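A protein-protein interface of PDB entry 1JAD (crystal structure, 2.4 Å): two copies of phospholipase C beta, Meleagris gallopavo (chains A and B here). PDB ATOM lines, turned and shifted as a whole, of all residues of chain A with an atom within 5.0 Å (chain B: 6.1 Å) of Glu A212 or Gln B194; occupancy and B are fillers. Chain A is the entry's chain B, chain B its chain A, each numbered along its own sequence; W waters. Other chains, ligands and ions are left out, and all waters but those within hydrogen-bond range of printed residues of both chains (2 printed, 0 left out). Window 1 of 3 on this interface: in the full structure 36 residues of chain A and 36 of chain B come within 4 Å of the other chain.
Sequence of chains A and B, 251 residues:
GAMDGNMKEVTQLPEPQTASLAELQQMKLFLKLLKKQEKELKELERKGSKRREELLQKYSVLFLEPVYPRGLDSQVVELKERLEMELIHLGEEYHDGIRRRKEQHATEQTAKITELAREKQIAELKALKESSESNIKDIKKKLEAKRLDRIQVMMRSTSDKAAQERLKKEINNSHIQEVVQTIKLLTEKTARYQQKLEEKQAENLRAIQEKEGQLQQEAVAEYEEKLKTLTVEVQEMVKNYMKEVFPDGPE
The side-chain amino group (NZ) of Lys B129 is in salt-bridge range of the side-chain carboxylate (OE2) of Glu A212, at 3.0 Å. OE2 of Glu A212 sits close to OE1 of Gln B194 (3.0 Å). The side-chain amide nitrogen (NE2) of Gln B194 lies within hydrogen-bond range of the side-chain amide oxygen (OE1) of Gln A216 (3.3 Å). NZ of Lys B129 lies close to OG1 of Thr A107.
OE1 of Gln B194 sits close to OE2 of Glu B198 (3.1 Å). The side-chain hydroxyl (OG1) of Thr A110 lies within hydrogen-bond range of the side-chain carboxylate (OE1) of Glu A212, 2.6 Å away. The side-chain carboxylate (OE2) of Glu A212 sits close to the side-chain amide oxygen (OE1) of Gln A216 (3.3 Å).
Among the printed residues, pairs that only touch across the chains: Gln A209 with Glu B198 (3.5 Å) and Gln A216 with Lys B129 (3.9 Å).
Glu A212 touches just these residues of chain B: Lys B129 and Gln B194. Of the printed residues of chain A, Gln B194 touches Glu A212 (3.0 Å) and Gln A216 (3.3 Å). Of the printed residues of chain A, Glu B198 touches Gln A209. Of the printed residues of chain B, Gln A216 touches Lys B129 and Gln B194. Printed residues of chain B within 4 Å of Thr A107: Lys B129 (2.4 Å). Printed residues of chain B within 4 Å of Gln A209: Glu B198. Printed residues of chain A within 4 Å of Lys B129: Thr A107 (2.4 Å), Glu A212 (3.0 Å) and Gln A216 (3.9 Å). Arg B192 touches none of the printed residues of chain A. Leu A215 touches none of the printed residues of chain B. The nearest residue of chain B that does not touch Glu A212 is Glu B198 (4.6 Å). The nearest printed residue of chain A that does not touch Gln B194 is Gln A209 (5.8 Å). The nearest printed residue of chain B that does not touch Gln A216 is Ala B191 (4.9 Å).
Printed residues of chain A that touch a printed residue of chain B: Thr A107, Gln A209, Glu A212 and Gln A216. Of the 15 printed residues of chain B, 3 touch a printed residue of chain A. Among the printed residues, 6 pairs touch across the chains. Among the printed residues, Asp or Glu carboxylates within 4 Å of a Lys or Arg side-chain nitrogen of the other chain: Glu A212 with Lys B129.
No position is printed for both chains.
Water W1 lies within hydrogen-bond range of OE1 of Gln A216 (2.9 Å), NZ of Lys B129 (3.0 Å) and OG1 of Thr A107 (3.2 Å). Water W2 lies within hydrogen-bond range of OE1 of Glu B198 (3.4 Å) and OE1 of Gln A209 (3.5 Å).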
ATOM      1  N   ALA A 106     -11.988  29.641 -23.066  1.00  0.00           N
ATOM      2  CA  ALA A 106     -12.180  28.336 -22.422  1.00  0.00           C
ATOM      3  C   ALA A 106     -11.745  28.385 -20.958  1.00  0.00           C
ATOM      4  O   ALA A 106     -12.426  27.855 -20.072  1.00  0.00           O
ATOM      5  CB  ALA A 106     -11.385  27.256 -23.163  1.00  0.00           C
ATOM      6  N   THR A 107     -10.604  29.024 -20.713  1.00  0.00           N
ATOM      7  CA  THR A 107     -10.065  29.146 -19.361  1.00  0.00           C
ATOM      8  C   THR A 107     -11.041  29.911 -18.470  1.00  0.00           C
ATOM      9  O   THR A 107     -11.391  29.449 -17.378  1.00  0.00           O
ATOM     10  CB  THR A 107      -8.710  29.882 -19.379  1.00  0.00           C
ATOM     11  OG1 THR A 107      -7.780  29.129 -20.156  1.00  0.00           O
ATOM     12  CG2 THR A 107      -8.153  30.051 -17.963  1.00  0.00           C
ATOM     13  N   THR A 110     -14.178  28.054 -17.550  1.00  0.00           N
ATOM     14  CA  THR A 110     -13.956  27.083 -16.472  1.00  0.00           C
ATOM     15  C   THR A 110     -13.925  27.775 -15.112  1.00  0.00           C
ATOM     16  O   THR A 110     -14.507  27.293 -14.143  1.00  0.00           O
ATOM     17  CB  THR A 110     -12.633  26.306 -16.658  1.00  0.00           C
ATOM     18  OG1 THR A 110     -12.802  25.342 -17.702  1.00  0.00           O
ATOM     19  CG2 THR A 110     -12.226  25.605 -15.365  1.00  0.00           C
ATOM     20  N   ILE A 208     -16.319  19.608 -16.381  1.00  0.00           N
ATOM     21  CA  ILE A 208     -15.998  21.009 -16.673  1.00  0.00           C
ATOM     22  C   ILE A 208     -14.672  21.035 -17.407  1.00  0.00           C
ATOM     23  O   ILE A 208     -14.509  21.719 -18.413  1.00  0.00           O
ATOM     24  CB  ILE A 208     -15.849  21.827 -15.356  1.00  0.00           C
ATOM     25  CG1 ILE A 208     -17.190  21.878 -14.622  1.00  0.00           C
ATOM     26  CG2 ILE A 208     -15.332  23.212 -15.653  1.00  0.00           C
ATOM     27  CD1 ILE A 208     -17.109  22.522 -13.256  1.00  0.00           C
ATOM     28  N   GLN A 209     -13.718  20.272 -16.889  1.00  0.00           N
ATOM     29  CA  GLN A 209     -12.392  20.215 -17.478  1.00  0.00           C
ATOM     30  C   GLN A 209     -12.432  19.517 -18.843  1.00  0.00           C
ATOM     31  O   GLN A 209     -11.699  19.877 -19.753  1.00  0.00           O
ATOM     32  CB  GLN A 209     -11.437  19.524 -16.494  1.00  0.00           C
ATOM     33  CG  GLN A 209     -11.452  20.187 -15.116  1.00  0.00           C
ATOM     34  CD  GLN A 209     -10.569  19.514 -14.087  1.00  0.00           C
ATOM     35  OE1 GLN A 209     -10.581  18.293 -13.933  1.00  0.00           O
ATOM     36  NE2 GLN A 209      -9.817  20.313 -13.348  1.00  0.00           N
ATOM     37  N   GLU A 210     -13.313  18.542 -19.006  1.00  0.00           N
ATOM     38  CA  GLU A 210     -13.401  17.864 -20.295  1.00  0.00           C
ATOM     39  C   GLU A 210     -13.945  18.819 -21.368  1.00  0.00           C
ATOM     40  O   GLU A 210     -13.542  18.763 -22.533  1.00  0.00           O
ATOM     41  CB  GLU A 210     -14.297  16.631 -20.191  1.00  0.00           C
ATOM     42  CG  GLU A 210     -14.161  15.690 -21.385  1.00  0.00           C
ATOM     43  CD  GLU A 210     -15.003  14.441 -21.246  1.00  0.00           C
ATOM     44  OE1 GLU A 210     -14.808  13.704 -20.248  1.00  0.00           O
ATOM     45  OE2 GLU A 210     -15.857  14.199 -22.129  1.00  0.00           O
ATOM     46  N   LYS A 211     -14.846  19.714 -20.959  1.00  0.00           N
ATOM     47  CA  LYS A 211     -15.437  20.692 -21.875  1.00  0.00           C
ATOM     48  C   LYS A 211     -14.352  21.657 -22.352  1.00  0.00           C
ATOM     49  O   LYS A 211     -14.242  21.966 -23.538  1.00  0.00           O
ATOM     50  CB  LYS A 211     -16.567  21.456 -21.172  1.00  0.00           C
ATOM     51  CG  LYS A 211     -17.284  22.477 -22.050  1.00  0.00           C
ATOM     52  CD  LYS A 211     -17.878  21.834 -23.316  1.00  0.00           C
ATOM     53  CE  LYS A 211     -18.655  22.839 -24.195  1.00  0.00           C
ATOM     54  NZ  LYS A 211     -19.929  23.334 -23.560  1.00  0.00           N
ATOM     55  N   GLU A 212     -13.537  22.123 -21.420  1.00  0.00           N
ATOM     56  CA  GLU A 212     -12.458  23.040 -21.757  1.00  0.00           C
ATOM     57  C   GLU A 212     -11.563  22.390 -22.825  1.00  0.00           C
ATOM     58  O   GLU A 212     -11.200  23.022 -23.840  1.00  0.00           O
ATOM     59  CB  GLU A 212     -11.646  23.341 -20.490  1.00  0.00           C
ATOM     60  CG  GLU A 212     -10.608  24.449 -20.634  1.00  0.00           C
ATOM     61  CD  GLU A 212      -9.801  24.607 -19.359  1.00  0.00           C
ATOM     62  OE1 GLU A 212     -10.427  24.532 -18.277  1.00  0.00           O
ATOM     63  OE2 GLU A 212      -8.561  24.813 -19.424  1.00  0.00           O
ATOM     64  N   GLY A 213     -11.209  21.122 -22.595  1.00  0.00           N
ATOM     65  CA  GLY A 213     -10.365  20.400 -23.535  1.00  0.00           C
ATOM     66  C   GLY A 213     -10.930  20.440 -24.949  1.00  0.00           C
ATOM     67  O   GLY A 213     -10.224  20.753 -25.914  1.00  0.00           O
ATOM     68  N   GLN A 214     -12.211  20.121 -25.076  1.00  0.00           N
ATOM     69  CA  GLN A 214     -12.867  20.149 -26.377  1.00  0.00           C
ATOM     70  C   GLN A 214     -12.746  21.538 -27.001  1.00  0.00           C
ATOM     71  O   GLN A 214     -12.437  21.680 -28.192  1.00  0.00           O
ATOM     72  CB  GLN A 214     -14.337  19.786 -26.219  1.00  0.00           C
ATOM     73  CG  GLN A 214     -14.557  18.411 -25.645  1.00  0.00           C
ATOM     74  CD  GLN A 214     -16.020  18.110 -25.435  1.00  0.00           C
ATOM     75  OE1 GLN A 214     -16.834  18.279 -26.349  1.00  0.00           O
ATOM     76  NE2 GLN A 214     -16.369  17.650 -24.234  1.00  0.00           N
ATOM     77  N   LEU A 215     -12.981  22.568 -26.191  1.00  0.00           N
ATOM     78  CA  LEU A 215     -12.904  23.951 -26.670  1.00  0.00           C
ATOM     79  C   LEU A 215     -11.472  24.218 -27.151  1.00  0.00           C
ATOM     80  O   LEU A 215     -11.255  24.762 -28.245  1.00  0.00           O
ATOM     81  CB  LEU A 215     -13.321  24.902 -25.531  1.00  0.00           C
ATOM     82  CG  LEU A 215     -14.567  25.784 -25.733  1.00  0.00           C
ATOM     83  CD1 LEU A 215     -15.599  25.118 -26.640  1.00  0.00           C
ATOM     84  CD2 LEU A 215     -15.164  26.104 -24.363  1.00  0.00           C
ATOM     85  N   GLN A 216     -10.491  23.827 -26.344  1.00  0.00           N
ATOM     86  CA  GLN A 216      -9.092  23.999 -26.735  1.00  0.00           C
ATOM     87  C   GLN A 216      -8.863  23.263 -28.063  1.00  0.00           C
ATOM     88  O   GLN A 216      -8.249  23.776 -29.003  1.00  0.00           O
ATOM     89  CB  GLN A 216      -8.174  23.418 -25.647  1.00  0.00           C
ATOM     90  CG  GLN A 216      -8.232  24.173 -24.313  1.00  0.00           C
ATOM     91  CD  GLN A 216      -7.315  23.588 -23.251  1.00  0.00           C
ATOM     92  OE1 GLN A 216      -7.028  24.232 -22.233  1.00  0.00           O
ATOM     93  NE2 GLN A 216      -6.866  22.350 -23.469  1.00  0.00           N
ATOM     94  N   GLN A 217      -9.395  22.056 -28.145  1.00  0.00           N
ATOM     95  CA  GLN A 217      -9.249  21.256 -29.345  1.00  0.00           C
ATOM     96  C   GLN A 217      -9.959  21.922 -30.541  1.00  0.00           C
ATOM     97  O   GLN A 217      -9.412  21.978 -31.646  1.00  0.00           O
ATOM     98  CB  GLN A 217      -9.783  19.853 -29.052  1.00  0.00           C
ATOM     99  CG  GLN A 217      -9.662  18.866 -30.183  1.00  0.00           C
ATOM    100  CD  GLN A 217     -10.167  17.482 -29.786  1.00  0.00           C
ATOM    101  OE1 GLN A 217     -10.289  16.589 -30.632  1.00  0.00           O
ATOM    102  NE2 GLN A 217     -10.455  17.296 -28.492  1.00  0.00           N
ATOM    103  N   PRO B  16       4.003  18.489 -14.317  1.00  0.00           N
ATOM    104  CA  PRO B  16       2.892  18.547 -13.367  1.00  0.00           C
ATOM    105  C   PRO B  16       3.244  18.324 -11.900  1.00  0.00           C
ATOM    106  O   PRO B  16       3.754  17.273 -11.534  1.00  0.00           O
ATOM    107  CB  PRO B  16       1.946  17.479 -13.906  1.00  0.00           C
ATOM    108  CG  PRO B  16       2.135  17.638 -15.389  1.00  0.00           C
ATOM    109  CD  PRO B  16       3.644  17.591 -15.431  1.00  0.00           C
ATOM    110  N   LEU B 125      -1.620  26.014 -13.261  1.00  0.00           N
ATOM    111  CA  LEU B 125      -2.311  25.947 -14.542  1.00  0.00           C
ATOM    112  C   LEU B 125      -1.955  27.145 -15.385  1.00  0.00           C
ATOM    113  O   LEU B 125      -1.863  27.049 -16.603  1.00  0.00           O
ATOM    114  CB  LEU B 125      -3.829  25.919 -14.355  1.00  0.00           C
ATOM    115  CG  LEU B 125      -4.491  24.709 -13.690  1.00  0.00           C
ATOM    116  CD1 LEU B 125      -5.983  24.979 -13.566  1.00  0.00           C
ATOM    117  CD2 LEU B 125      -4.247  23.449 -14.512  1.00  0.00           C
ATOM    118  N   LEU B 128       1.681  26.668 -16.756  1.00  0.00           N
ATOM    119  CA  LEU B 128       1.743  25.688 -17.836  1.00  0.00           C
ATOM    120  C   LEU B 128       1.287  26.335 -19.145  1.00  0.00           C
ATOM    121  O   LEU B 128       1.984  26.266 -20.160  1.00  0.00           O
ATOM    122  CB  LEU B 128       0.866  24.482 -17.496  1.00  0.00           C
ATOM    123  CG  LEU B 128       0.672  23.386 -18.542  1.00  0.00           C
ATOM    124  CD1 LEU B 128       2.020  22.747 -18.925  1.00  0.00           C
ATOM    125  CD2 LEU B 128      -0.276  22.344 -17.968  1.00  0.00           C
ATOM    126  N   LYS B 129       0.130  26.997 -19.105  1.00  0.00           N
ATOM    127  CA  LYS B 129      -0.414  27.670 -20.279  1.00  0.00           C
ATOM    128  C   LYS B 129       0.486  28.756 -20.857  1.00  0.00           C
ATOM    129  O   LYS B 129       0.639  28.829 -22.080  1.00  0.00           O
ATOM    130  CB  LYS B 129      -1.794  28.263 -19.976  1.00  0.00           C
ATOM    131  CG  LYS B 129      -2.827  27.222 -19.606  1.00  0.00           C
ATOM    132  CD  LYS B 129      -4.249  27.760 -19.701  1.00  0.00           C
ATOM    133  CE  LYS B 129      -5.250  26.664 -19.350  1.00  0.00           C
ATOM    134  NZ  LYS B 129      -6.642  27.119 -19.568  1.00  0.00           N
ATOM    135  N   LYS B 189       0.627  17.995 -26.513  1.00  0.00           N
ATOM    136  CA  LYS B 189       1.432  17.723 -25.329  1.00  0.00           C
ATOM    137  C   LYS B 189       0.920  18.593 -24.163  1.00  0.00           C
ATOM    138  O   LYS B 189       0.741  18.103 -23.045  1.00  0.00           O
ATOM    139  CB  LYS B 189       2.903  18.016 -25.625  1.00  0.00           C
ATOM    140  CG  LYS B 189       3.863  17.704 -24.482  1.00  0.00           C
ATOM    141  CD  LYS B 189       5.306  18.002 -24.899  1.00  0.00           C
ATOM    142  CE  LYS B 189       6.279  17.639 -23.787  1.00  0.00           C
ATOM    143  NZ  LYS B 189       7.693  17.975 -24.117  1.00  0.00           N
ATOM    144  N   THR B 190       0.674  19.881 -24.412  1.00  0.00           N
ATOM    145  CA  THR B 190       0.153  20.746 -23.342  1.00  0.00           C
ATOM    146  C   THR B 190      -1.137  20.130 -22.791  1.00  0.00           C
ATOM    147  O   THR B 190      -1.390  20.158 -21.590  1.00  0.00           O
ATOM    148  CB  THR B 190      -0.125  22.172 -23.852  1.00  0.00           C
ATOM    149  OG1 THR B 190       1.090  22.739 -24.369  1.00  0.00           O
ATOM    150  CG2 THR B 190      -0.642  23.049 -22.723  1.00  0.00           C
ATOM    151  N   ALA B 191      -1.953  19.546 -23.658  1.00  0.00           N
ATOM    152  CA  ALA B 191      -3.171  18.912 -23.182  1.00  0.00           C
ATOM    153  C   ALA B 191      -2.835  17.738 -22.249  1.00  0.00           C
ATOM    154  O   ALA B 191      -3.516  17.519 -21.230  1.00  0.00           O
ATOM    155  CB  ALA B 191      -3.990  18.428 -24.344  1.00  0.00           C
ATOM    156  N   ARG B 192      -1.793  16.976 -22.580  1.00  0.00           N
ATOM    157  CA  ARG B 192      -1.423  15.852 -21.721  1.00  0.00           C
ATOM    158  C   ARG B 192      -0.904  16.366 -20.383  1.00  0.00           C
ATOM    159  O   ARG B 192      -1.275  15.850 -19.336  1.00  0.00           O
ATOM    160  CB  ARG B 192      -0.371  14.948 -22.402  1.00  0.00           C
ATOM    161  CG  ARG B 192       0.247  13.877 -21.485  1.00  0.00           C
ATOM    162  CD  ARG B 192       0.917  12.738 -22.269  1.00  0.00           C
ATOM    163  NE  ARG B 192       1.894  13.232 -23.240  1.00  0.00           N
ATOM    164  CZ  ARG B 192       3.143  13.545 -22.929  1.00  0.00           C
ATOM    165  NH1 ARG B 192       3.550  13.401 -21.677  1.00  0.00           N
ATOM    166  NH2 ARG B 192       3.964  14.040 -23.855  1.00  0.00           N
ATOM    167  N   TYR B 193      -0.047  17.380 -20.408  1.00  0.00           N
ATOM    168  CA  TYR B 193       0.465  17.935 -19.155  1.00  0.00           C
ATOM    169  C   TYR B 193      -0.632  18.560 -18.293  1.00  0.00           C
ATOM    170  O   TYR B 193      -0.587  18.469 -17.062  1.00  0.00           O
ATOM    171  CB  TYR B 193       1.550  18.975 -19.430  1.00  0.00           C
ATOM    172  CG  TYR B 193       2.942  18.382 -19.612  1.00  0.00           C
ATOM    173  CD1 TYR B 193       3.183  17.368 -20.555  1.00  0.00           C
ATOM    174  CD2 TYR B 193       4.019  18.837 -18.841  1.00  0.00           C
ATOM    175  CE1 TYR B 193       4.454  16.824 -20.725  1.00  0.00           C
ATOM    176  CE2 TYR B 193       5.294  18.302 -19.003  1.00  0.00           C
ATOM    177  CZ  TYR B 193       5.505  17.301 -19.945  1.00  0.00           C
ATOM    178  OH  TYR B 193       6.772  16.796 -20.125  1.00  0.00           O
ATOM    179  N   GLN B 194      -1.627  19.182 -18.919  1.00  0.00           N
ATOM    180  CA  GLN B 194      -2.686  19.808 -18.129  1.00  0.00           C
ATOM    181  C   GLN B 194      -3.580  18.756 -17.483  1.00  0.00           C
ATOM    182  O   GLN B 194      -3.939  18.854 -16.311  1.00  0.00           O
ATOM    183  CB  GLN B 194      -3.518  20.774 -18.984  1.00  0.00           C
ATOM    184  CG  GLN B 194      -4.722  21.313 -18.232  1.00  0.00           C
ATOM    185  CD  GLN B 194      -5.541  22.336 -19.008  1.00  0.00           C
ATOM    186  OE1 GLN B 194      -6.689  22.589 -18.664  1.00  0.00           O
ATOM    187  NE2 GLN B 194      -4.955  22.943 -20.027  1.00  0.00           N
ATOM    188  N   GLN B 195      -3.917  17.728 -18.250  1.00  0.00           N
ATOM    189  CA  GLN B 195      -4.746  16.648 -17.758  1.00  0.00           C
ATOM    190  C   GLN B 195      -4.132  15.987 -16.526  1.00  0.00           C
ATOM    191  O   GLN B 195      -4.812  15.748 -15.524  1.00  0.00           O
ATOM    192  CB  GLN B 195      -4.948  15.640 -18.893  1.00  0.00           C
ATOM    193  CG  GLN B 195      -5.497  14.281 -18.493  1.00  0.00           C
ATOM    194  CD  GLN B 195      -4.424  13.387 -17.882  1.00  0.00           C
ATOM    195  OE1 GLN B 195      -3.442  13.022 -18.549  1.00  0.00           O
ATOM    196  NE2 GLN B 195      -4.596  13.044 -16.606  1.00  0.00           N
ATOM    197  N   LYS B 196      -2.839  15.698 -16.592  1.00  0.00           N
ATOM    198  CA  LYS B 196      -2.147  15.045 -15.488  1.00  0.00           C
ATOM    199  C   LYS B 196      -2.123  16.000 -14.287  1.00  0.00           C
ATOM    200  O   LYS B 196      -2.318  15.593 -13.139  1.00  0.00           O
ATOM    201  CB  LYS B 196      -0.712  14.707 -15.915  1.00  0.00           C
ATOM    202  CG  LYS B 196      -0.097  13.461 -15.266  1.00  0.00           C
ATOM    203  CD  LYS B 196      -0.057  13.499 -13.749  1.00  0.00           C
ATOM    204  CE  LYS B 196       0.495  12.175 -13.191  1.00  0.00           C
ATOM    205  NZ  LYS B 196      -0.289  10.962 -13.631  1.00  0.00           N
ATOM    206  N   LEU B 197      -1.890  17.275 -14.572  1.00  0.00           N
ATOM    207  CA  LEU B 197      -1.828  18.304 -13.540  1.00  0.00           C
ATOM    208  C   LEU B 197      -3.152  18.428 -12.787  1.00  0.00           C
ATOM    209  O   LEU B 197      -3.187  18.448 -11.555  1.00  0.00           O
ATOM    210  CB  LEU B 197      -1.455  19.645 -14.187  1.00  0.00           C
ATOM    211  CG  LEU B 197      -1.197  20.849 -13.281  1.00  0.00           C
ATOM    212  CD1 LEU B 197      -0.612  22.002 -14.075  1.00  0.00           C
ATOM    213  CD2 LEU B 197      -2.491  21.262 -12.635  1.00  0.00           C
ATOM    214  N   GLU B 198      -4.248  18.513 -13.527  1.00  0.00           N
ATOM    215  CA  GLU B 198      -5.553  18.643 -12.898  1.00  0.00           C
ATOM    216  C   GLU B 198      -5.832  17.386 -12.106  1.00  0.00           C
ATOM    217  O   GLU B 198      -6.539  17.398 -11.100  1.00  0.00           O
ATOM    218  CB  GLU B 198      -6.633  18.854 -13.961  1.00  0.00           C
ATOM    219  CG  GLU B 198      -6.311  19.973 -14.915  1.00  0.00           C
ATOM    220  CD  GLU B 198      -7.432  20.270 -15.876  1.00  0.00           C
ATOM    221  OE1 GLU B 198      -7.945  19.320 -16.506  1.00  0.00           O
ATOM    222  OE2 GLU B 198      -7.795  21.463 -16.015  1.00  0.00           O
ATOM    223  N   GLU B 199      -5.243  16.294 -12.557  1.00  0.00           N
ATOM    224  CA  GLU B 199      -5.426  15.011 -11.902  1.00  0.00           C
ATOM    225  C   GLU B 199      -4.813  15.012 -10.499  1.00  0.00           C
ATOM    226  O   GLU B 199      -5.417  14.527  -9.553  1.00  0.00           O
ATOM    227  CB  GLU B 199      -4.795  13.929 -12.764  1.00  0.00           C
ATOM    228  CG  GLU B 199      -5.166  12.526 -12.383  1.00  0.00           C
ATOM    229  CD  GLU B 199      -4.525  11.518 -13.312  1.00  0.00           C
ATOM    230  OE1 GLU B 199      -3.289  11.338 -13.236  1.00  0.00           O
ATOM    231  OE2 GLU B 199      -5.255  10.926 -14.135  1.00  0.00           O
HETATM  232  O   HOH W   1      -7.103  27.102 -22.506  1.00  0.00           O
HETATM  233  O   HOH W   2      -9.034  16.157 -16.197  1.00  0.00           O
